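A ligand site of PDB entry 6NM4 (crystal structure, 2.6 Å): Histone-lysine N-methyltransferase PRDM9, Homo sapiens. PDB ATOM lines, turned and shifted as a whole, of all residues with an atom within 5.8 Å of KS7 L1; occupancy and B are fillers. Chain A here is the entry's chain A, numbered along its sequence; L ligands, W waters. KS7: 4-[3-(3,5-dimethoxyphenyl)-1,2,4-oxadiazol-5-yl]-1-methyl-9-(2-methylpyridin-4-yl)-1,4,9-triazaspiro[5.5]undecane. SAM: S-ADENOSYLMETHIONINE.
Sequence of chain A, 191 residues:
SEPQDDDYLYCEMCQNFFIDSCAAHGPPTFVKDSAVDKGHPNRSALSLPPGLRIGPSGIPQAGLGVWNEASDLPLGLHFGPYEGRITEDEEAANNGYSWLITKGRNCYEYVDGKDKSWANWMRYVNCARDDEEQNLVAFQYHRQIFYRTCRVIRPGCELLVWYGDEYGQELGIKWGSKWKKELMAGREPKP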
ATOM      1  N   TYR A  82      -5.121  -7.034  22.199  1.00  0.00           N
ATOM      2  CA  TYR A  82      -4.200  -6.998  21.076  1.00  0.00           C
ATOM      3  C   TYR A  82      -5.068  -6.846  19.838  1.00  0.00           C
ATOM      4  O   TYR A  82      -5.937  -7.669  19.587  1.00  0.00           O
ATOM      5  CB  TYR A  82      -3.364  -8.284  21.026  1.00  0.00           C
ATOM      6  CG  TYR A  82      -2.167  -8.279  20.070  1.00  0.00           C
ATOM      7  CD1 TYR A  82      -2.300  -8.677  18.766  1.00  0.00           C
ATOM      8  CD2 TYR A  82      -0.894  -7.911  20.504  1.00  0.00           C
ATOM      9  CE1 TYR A  82      -1.220  -8.700  17.900  1.00  0.00           C
ATOM     10  CE2 TYR A  82       0.203  -7.948  19.661  1.00  0.00           C
ATOM     11  CZ  TYR A  82       0.021  -8.347  18.342  1.00  0.00           C
ATOM     12  OH  TYR A  82       1.071  -8.397  17.457  1.00  0.00           O
ATOM     13  N   ASN A  94       3.707 -17.026  12.947  1.00  0.00           N
ATOM     14  CA  ASN A  94       5.162 -16.822  12.815  1.00  0.00           C
ATOM     15  C   ASN A  94       5.518 -15.864  11.671  1.00  0.00           C
ATOM     16  O   ASN A  94       6.464 -16.091  10.938  1.00  0.00           O
ATOM     17  CB  ASN A  94       5.912 -18.166  12.613  1.00  0.00           C
ATOM     18  CG  ASN A  94       5.858 -19.059  13.853  1.00  0.00           C
ATOM     19  OD1 ASN A  94       4.818 -19.158  14.514  1.00  0.00           O
ATOM     20  ND2 ASN A  94       6.979 -19.723  14.154  1.00  0.00           N
ATOM     21  N   GLY A  96       5.834 -12.956  13.095  1.00  0.00           N
ATOM     22  CA  GLY A  96       6.348 -12.098  14.149  1.00  0.00           C
ATOM     23  C   GLY A  96       5.279 -11.379  14.959  1.00  0.00           C
ATOM     24  O   GLY A  96       5.561 -10.935  16.067  1.00  0.00           O
ATOM     25  N   TYR A  97       4.052 -11.249  14.443  1.00  0.00           N
ATOM     26  CA  TYR A  97       3.044 -10.347  15.041  1.00  0.00           C
ATOM     27  C   TYR A  97       1.665 -11.001  15.269  1.00  0.00           C
ATOM     28  O   TYR A  97       0.667 -10.293  15.509  1.00  0.00           O
ATOM     29  CB  TYR A  97       2.918  -9.088  14.172  1.00  0.00           C
ATOM     30  CG  TYR A  97       4.223  -8.320  14.027  1.00  0.00           C
ATOM     31  CD1 TYR A  97       5.126  -8.657  13.024  1.00  0.00           C
ATOM     32  CD2 TYR A  97       4.543  -7.282  14.874  1.00  0.00           C
ATOM     33  CE1 TYR A  97       6.326  -7.974  12.871  1.00  0.00           C
ATOM     34  CE2 TYR A  97       5.730  -6.578  14.742  1.00  0.00           C
ATOM     35  CZ  TYR A  97       6.623  -6.944  13.734  1.00  0.00           C
ATOM     36  OH  TYR A  97       7.817  -6.269  13.581  1.00  0.00           O
ATOM     37  N   SER A  98       1.605 -12.323  15.205  1.00  0.00           N
ATOM     38  CA  SER A  98       0.323 -13.031  15.292  1.00  0.00           C
ATOM     39  C   SER A  98       0.230 -13.800  16.594  1.00  0.00           C
ATOM     40  O   SER A  98       1.196 -14.406  17.024  1.00  0.00           O
ATOM     41  CB  SER A  98       0.174 -13.999  14.139  1.00  0.00           C
ATOM     42  OG  SER A  98       0.308 -13.323  12.906  1.00  0.00           O
ATOM     43  N   TRP A  99      -0.944 -13.751  17.215  1.00  0.00           N
ATOM     44  CA  TRP A  99      -1.225 -14.542  18.380  1.00  0.00           C
ATOM     45  C   TRP A  99      -2.360 -15.503  18.042  1.00  0.00           C
ATOM     46  O   TRP A  99      -3.242 -15.219  17.234  1.00  0.00           O
ATOM     47  CB  TRP A  99      -1.724 -13.674  19.511  1.00  0.00           C
ATOM     48  CG  TRP A  99      -0.712 -12.882  20.242  1.00  0.00           C
ATOM     49  CD1 TRP A  99      -0.624 -11.530  20.271  1.00  0.00           C
ATOM     50  CD2 TRP A  99       0.285 -13.362  21.139  1.00  0.00           C
ATOM     51  NE1 TRP A  99       0.383 -11.131  21.099  1.00  0.00           N
ATOM     52  CE2 TRP A  99       0.968 -12.241  21.644  1.00  0.00           C
ATOM     53  CE3 TRP A  99       0.696 -14.628  21.548  1.00  0.00           C
ATOM     54  CZ2 TRP A  99       2.041 -12.346  22.545  1.00  0.00           C
ATOM     55  CZ3 TRP A  99       1.753 -14.733  22.443  1.00  0.00           C
ATOM     56  CH2 TRP A  99       2.408 -13.605  22.939  1.00  0.00           C
ATOM     57  N   CYS A 127       9.458 -10.058  23.526  1.00  0.00           N
ATOM     58  CA  CYS A 127       9.315 -11.223  24.399  1.00  0.00           C
ATOM     59  C   CYS A 127      10.446 -11.359  25.391  1.00  0.00           C
ATOM     60  O   CYS A 127      11.601 -11.192  25.038  1.00  0.00           O
ATOM     61  CB  CYS A 127       9.261 -12.502  23.584  1.00  0.00           C
ATOM     62  SG  CYS A 127       7.783 -12.584  22.557  1.00  0.00           S
ATOM     63  N   ALA A 128      10.103 -11.665  26.632  1.00  0.00           N
ATOM     64  CA  ALA A 128      11.092 -12.068  27.631  1.00  0.00           C
ATOM     65  C   ALA A 128      11.889 -13.266  27.146  1.00  0.00           C
ATOM     66  O   ALA A 128      11.371 -14.129  26.423  1.00  0.00           O
ATOM     67  CB  ALA A 128      10.415 -12.407  28.940  1.00  0.00           C
ATOM     68  N   ARG A 129      13.170 -13.296  27.539  1.00  0.00           N
ATOM     69  CA  ARG A 129      14.045 -14.431  27.253  1.00  0.00           C
ATOM     70  C   ARG A 129      14.033 -15.463  28.382  1.00  0.00           C
ATOM     71  O   ARG A 129      14.350 -16.619  28.162  1.00  0.00           O
ATOM     72  CB  ARG A 129      15.471 -13.958  27.022  1.00  0.00           C
ATOM     73  CG  ARG A 129      15.609 -13.124  25.768  1.00  0.00           C
ATOM     74  CD  ARG A 129      16.944 -12.417  25.704  1.00  0.00           C
ATOM     75  NE  ARG A 129      17.099 -11.438  26.782  1.00  0.00           N
ATOM     76  CZ  ARG A 129      18.116 -10.569  26.860  1.00  0.00           C
ATOM     77  NH1 ARG A 129      19.085 -10.549  25.936  1.00  0.00           N
ATOM     78  NH2 ARG A 129      18.162  -9.721  27.884  1.00  0.00           N
ATOM     79  N   ASP A 130      13.633 -15.037  29.569  1.00  0.00           N
ATOM     80  CA  ASP A 130      13.603 -15.909  30.729  1.00  0.00           C
ATOM     81  C   ASP A 130      12.586 -15.393  31.737  1.00  0.00           C
ATOM     82  O   ASP A 130      12.154 -14.233  31.658  1.00  0.00           O
ATOM     83  CB  ASP A 130      15.004 -16.045  31.368  1.00  0.00           C
ATOM     84  CG  ASP A 130      15.615 -14.698  31.778  1.00  0.00           C
ATOM     85  OD1 ASP A 130      15.007 -13.951  32.582  1.00  0.00           O
ATOM     86  OD2 ASP A 130      16.748 -14.376  31.312  1.00  0.00           O
ATOM     87  N   ASP A 131      12.235 -16.238  32.680  1.00  0.00           N
ATOM     88  CA  ASP A 131      11.232 -15.893  33.689  1.00  0.00           C
ATOM     89  C   ASP A 131      11.637 -14.668  34.525  1.00  0.00           C
ATOM     90  O   ASP A 131      10.791 -13.902  34.959  1.00  0.00           O
ATOM     91  CB  ASP A 131      10.970 -17.108  34.603  1.00  0.00           C
ATOM     92  CG  ASP A 131      10.446 -18.348  33.838  1.00  0.00           C
ATOM     93  OD1 ASP A 131       9.848 -18.197  32.744  1.00  0.00           O
ATOM     94  OD2 ASP A 131      10.648 -19.479  34.352  1.00  0.00           O
ATOM     95  N   GLN A 134      10.898 -11.403  32.620  1.00  0.00           N
ATOM     96  CA  GLN A 134       9.490 -11.343  32.205  1.00  0.00           C
ATOM     97  C   GLN A 134       8.667 -10.572  33.216  1.00  0.00           C
ATOM     98  O   GLN A 134       8.653 -10.914  34.392  1.00  0.00           O
ATOM     99  CB  GLN A 134       8.892 -12.744  32.072  1.00  0.00           C
ATOM    100  CG  GLN A 134       7.406 -12.755  31.819  1.00  0.00           C
ATOM    101  CD  GLN A 134       6.820 -14.137  31.544  1.00  0.00           C
ATOM    102  OE1 GLN A 134       7.460 -15.168  31.783  1.00  0.00           O
ATOM    103  NE2 GLN A 134       5.586 -14.161  31.041  1.00  0.00           N
ATOM    104  N   TYR A 147      -2.259  -8.578  27.910  1.00  0.00           N
ATOM    105  CA  TYR A 147      -0.994  -8.754  28.620  1.00  0.00           C
ATOM    106  C   TYR A 147      -1.208  -8.258  30.046  1.00  0.00           C
ATOM    107  O   TYR A 147      -1.621  -7.106  30.223  1.00  0.00           O
ATOM    108  CB  TYR A 147       0.105  -7.911  27.976  1.00  0.00           C
ATOM    109  CG  TYR A 147       0.511  -8.248  26.549  1.00  0.00           C
ATOM    110  CD1 TYR A 147       0.137  -9.427  25.924  1.00  0.00           C
ATOM    111  CD2 TYR A 147       1.286  -7.369  25.835  1.00  0.00           C
ATOM    112  CE1 TYR A 147       0.538  -9.703  24.626  1.00  0.00           C
ATOM    113  CE2 TYR A 147       1.689  -7.634  24.551  1.00  0.00           C
ATOM    114  CZ  TYR A 147       1.306  -8.794  23.935  1.00  0.00           C
ATOM    115  OH  TYR A 147       1.745  -9.024  22.647  1.00  0.00           O
ATOM    116  N   TRP A 162       5.699 -13.035  27.893  1.00  0.00           N
ATOM    117  CA  TRP A 162       5.650 -14.414  27.422  1.00  0.00           C
ATOM    118  C   TRP A 162       4.333 -14.975  27.952  1.00  0.00           C
ATOM    119  O   TRP A 162       3.520 -14.248  28.516  1.00  0.00           O
ATOM    120  CB  TRP A 162       6.888 -15.192  27.901  1.00  0.00           C
ATOM    121  CG  TRP A 162       7.128 -16.487  27.150  1.00  0.00           C
ATOM    122  CD1 TRP A 162       7.127 -17.755  27.665  1.00  0.00           C
ATOM    123  CD2 TRP A 162       7.374 -16.624  25.740  1.00  0.00           C
ATOM    124  NE1 TRP A 162       7.345 -18.671  26.668  1.00  0.00           N
ATOM    125  CE2 TRP A 162       7.503 -18.014  25.476  1.00  0.00           C
ATOM    126  CE3 TRP A 162       7.495 -15.721  24.677  1.00  0.00           C
ATOM    127  CZ2 TRP A 162       7.764 -18.522  24.195  1.00  0.00           C
ATOM    128  CZ3 TRP A 162       7.769 -16.227  23.392  1.00  0.00           C
ATOM    129  CH2 TRP A 162       7.888 -17.622  23.164  1.00  0.00           C
ATOM    130  N   TYR A 163       4.107 -16.259  27.739  1.00  0.00           N
ATOM    131  CA  TYR A 163       2.836 -16.906  28.006  1.00  0.00           C
ATOM    132  C   TYR A 163       2.988 -18.252  28.674  1.00  0.00           C
ATOM    133  O   TYR A 163       4.104 -18.737  28.864  1.00  0.00           O
ATOM    134  CB  TYR A 163       2.082 -17.104  26.690  1.00  0.00           C
ATOM    135  CG  TYR A 163       2.821 -17.925  25.662  1.00  0.00           C
ATOM    136  CD1 TYR A 163       2.808 -19.307  25.707  1.00  0.00           C
ATOM    137  CD2 TYR A 163       3.551 -17.313  24.656  1.00  0.00           C
ATOM    138  CE1 TYR A 163       3.476 -20.055  24.748  1.00  0.00           C
ATOM    139  CE2 TYR A 163       4.229 -18.055  23.706  1.00  0.00           C
ATOM    140  CZ  TYR A 163       4.162 -19.436  23.749  1.00  0.00           C
ATOM    141  OH  TYR A 163       4.849 -20.148  22.805  1.00  0.00           O
ATOM    142  N   TYR A 167      -2.876 -19.649  27.339  1.00  0.00           N
ATOM    143  CA  TYR A 167      -2.749 -19.174  25.984  1.00  0.00           C
ATOM    144  C   TYR A 167      -2.590 -20.318  24.997  1.00  0.00           C
ATOM    145  O   TYR A 167      -1.944 -21.330  25.294  1.00  0.00           O
ATOM    146  CB  TYR A 167      -1.535 -18.255  25.850  1.00  0.00           C
ATOM    147  CG  TYR A 167      -1.145 -18.101  24.405  1.00  0.00           C
ATOM    148  CD1 TYR A 167      -1.878 -17.257  23.572  1.00  0.00           C
ATOM    149  CD2 TYR A 167      -0.099 -18.847  23.849  1.00  0.00           C
ATOM    150  CE1 TYR A 167      -1.576 -17.142  22.236  1.00  0.00           C
ATOM    151  CE2 TYR A 167       0.223 -18.721  22.509  1.00  0.00           C
ATOM    152  CZ  TYR A 167      -0.512 -17.864  21.703  1.00  0.00           C
ATOM    153  OH  TYR A 167      -0.225 -17.725  20.357  1.00  0.00           O
HETATM  154  C4  KS7 L   1       3.357 -17.125  19.759  1.00  0.00           C
HETATM  155  C5  KS7 L   1       6.597 -15.503  19.572  1.00  0.00           C
HETATM  156  C6  KS7 L   1       7.228 -14.277  19.409  1.00  0.00           C
HETATM  157  N1  KS7 L   1      11.833 -15.536  19.508  1.00  0.00           N
HETATM  158  C7  KS7 L   1       8.716 -14.198  19.394  1.00  0.00           C
HETATM  159  C8  KS7 L   1      10.716 -14.832  19.426  1.00  0.00           C
HETATM  160  N2  KS7 L   1      11.062 -17.952  24.056  1.00  0.00           N
HETATM  161  C9  KS7 L   1      11.739 -16.920  19.957  1.00  0.00           C
HETATM  162  C10 KS7 L   1      12.211 -17.054  21.445  1.00  0.00           C
HETATM  163  C11 KS7 L   1      11.389 -16.146  22.363  1.00  0.00           C
HETATM  164  C12 KS7 L   1      11.308 -16.522  23.841  1.00  0.00           C
HETATM  165  N3  KS7 L   1      10.519 -19.126  28.066  1.00  0.00           N
HETATM  166  C13 KS7 L   1      10.884 -18.354  25.396  1.00  0.00           C
HETATM  167  C14 KS7 L   1      10.783 -17.412  26.424  1.00  0.00           C
HETATM  168  C15 KS7 L   1      10.600 -17.822  27.741  1.00  0.00           C
HETATM  169  N4  KS7 L   1      13.692 -16.772  21.381  1.00  0.00           N
HETATM  170  C21 KS7 L   1      14.411 -16.398  22.607  1.00  0.00           C
HETATM  171  C20 KS7 L   1      11.939 -18.530  21.812  1.00  0.00           C
HETATM  172  C19 KS7 L   1      12.030 -18.772  23.309  1.00  0.00           C
HETATM  173  C18 KS7 L   1      10.790 -19.698  25.747  1.00  0.00           C
HETATM  174  C17 KS7 L   1      10.618 -20.031  27.083  1.00  0.00           C
HETATM  175  C16 KS7 L   1      10.501 -16.834  28.859  1.00  0.00           C
HETATM  176  C22 KS7 L   1      14.155 -15.988  20.214  1.00  0.00           C
HETATM  177  C23 KS7 L   1      13.124 -14.919  19.832  1.00  0.00           C
HETATM  178  O2  KS7 L   1      10.740 -13.513  19.171  1.00  0.00           O
HETATM  179  N   KS7 L   1       9.367 -13.095  19.156  1.00  0.00           N
HETATM  180  N5  KS7 L   1       9.505 -15.309  19.566  1.00  0.00           N
HETATM  181  C3  KS7 L   1       5.210 -15.590  19.492  1.00  0.00           C
HETATM  182  O1  KS7 L   1       4.766 -16.866  19.737  1.00  0.00           O
HETATM  183  C2  KS7 L   1       4.445 -14.457  19.240  1.00  0.00           C
HETATM  184  C24 KS7 L   1       6.468 -13.136  19.180  1.00  0.00           C
HETATM  185  C1  KS7 L   1       5.085 -13.226  19.109  1.00  0.00           C
HETATM  186  O   KS7 L   1       4.515 -12.001  18.945  1.00  0.00           O
HETATM  187  C   KS7 L   1       3.085 -11.910  18.900  1.00  0.00           C
HETATM  188  N   SAM L   2      10.832  -5.650  18.109  1.00  0.00           N
HETATM  189  CA  SAM L   2       9.637  -5.756  17.302  1.00  0.00           C
HETATM  190  C   SAM L   2       9.603  -4.670  16.261  1.00  0.00           C
HETATM  191  O   SAM L   2      10.493  -3.806  16.241  1.00  0.00           O
HETATM  192  OXT SAM L   2       8.680  -4.674  15.428  1.00  0.00           O
HETATM  193  CB  SAM L   2       8.400  -5.720  18.230  1.00  0.00           C
HETATM  194  CG  SAM L   2       8.094  -7.104  18.779  1.00  0.00           C
HETATM  195  SD  SAM L   2       7.341  -8.083  17.645  1.00  0.00           S
HETATM  196  CE  SAM L   2       5.830  -8.457  18.244  1.00  0.00           C
HETATM  197  C5' SAM L   2       8.110  -9.549  17.368  1.00  0.00           C
HETATM  198  C4' SAM L   2       9.392  -9.472  16.544  1.00  0.00           C
HETATM  199  O4' SAM L   2      10.416  -8.749  17.240  1.00  0.00           O
HETATM  200  C3' SAM L   2       9.948 -10.859  16.247  1.00  0.00           C
HETATM  201  O3' SAM L   2       9.608 -11.355  14.958  1.00  0.00           O
HETATM  202  C2' SAM L   2      11.442 -10.663  16.286  1.00  0.00           C
HETATM  203  O2' SAM L   2      11.857 -10.345  14.945  1.00  0.00           O
HETATM  204  C1' SAM L   2      11.606  -9.529  17.284  1.00  0.00           C
HETATM  205  N9  SAM L   2      11.742 -10.021  18.670  1.00  0.00           N
HETATM  206  C8  SAM L   2      10.800  -9.977  19.657  1.00  0.00           C
HETATM  207  N7  SAM L   2      11.254 -10.519  20.813  1.00  0.00           N
HETATM  208  C5  SAM L   2      12.527 -10.919  20.561  1.00  0.00           C
HETATM  209  C6  SAM L   2      13.595 -11.583  21.334  1.00  0.00           C
HETATM  210  N6  SAM L   2      13.377 -11.905  22.624  1.00  0.00           N
HETATM  211  N1  SAM L   2      14.775 -11.832  20.708  1.00  0.00           N
HETATM  212  C2  SAM L   2      15.002 -11.504  19.428  1.00  0.00           C
HETATM  213  N3  SAM L   2      14.066 -10.911  18.663  1.00  0.00           N
HETATM  214  C4  SAM L   2      12.844 -10.603  19.167  1.00  0.00           C
HETATM  215  O   HOH W   1      10.221 -19.965  30.537  1.00  0.00           O
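The backbone carbonyl oxygen (O) of Gly 96 lies close to an oxygen (O) of KS7 L1, at 3.2 Å. Merely in contact with KS7 L1: Ala 128, Trp 99, Ser 98, Asp 130, Tyr 167 and Arg 129. Hydrophobic or aromatic side chains within 4 Å of KS7 L1: Trp 99 and Trp 162. Of the 16 residues printed, 9 come within 4 Å of KS7 L1. The nearest printed residue that does not touch KS7 L1 is Tyr 97 (4.003 Å).
SG of Cys 127 sits close to N of KS7 L1 (3.8 Å). O of Cys 127 sits at hydrogen-bond distance from N6 of SAM L2 (3.1 Å). OXT of SAM L2 is in hydrogen-bond range of OH of Tyr 97 (2.6 Å). NE1 of Trp 162 sits at hydrogen-bond distance from N3 of KS7 L1 (3.5 Å). A nitrogen (N7) of SAM L2 is in hydrogen-bond range of the backbone NH (N) of Cys 127 (3.3 Å).
O of Trp 162 sits at hydrogen-bond distance from NE2 of Gln 134, at 3.3 Å. OH of Tyr 147 is in hydrogen-bond range of NE1 of Trp 99 (2.9 Å).
Water W1 lies within hydrogen-bond range of N3 of KS7 L1 (2.6 Å) and OD1 of Asp 131 (2.9 Å).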
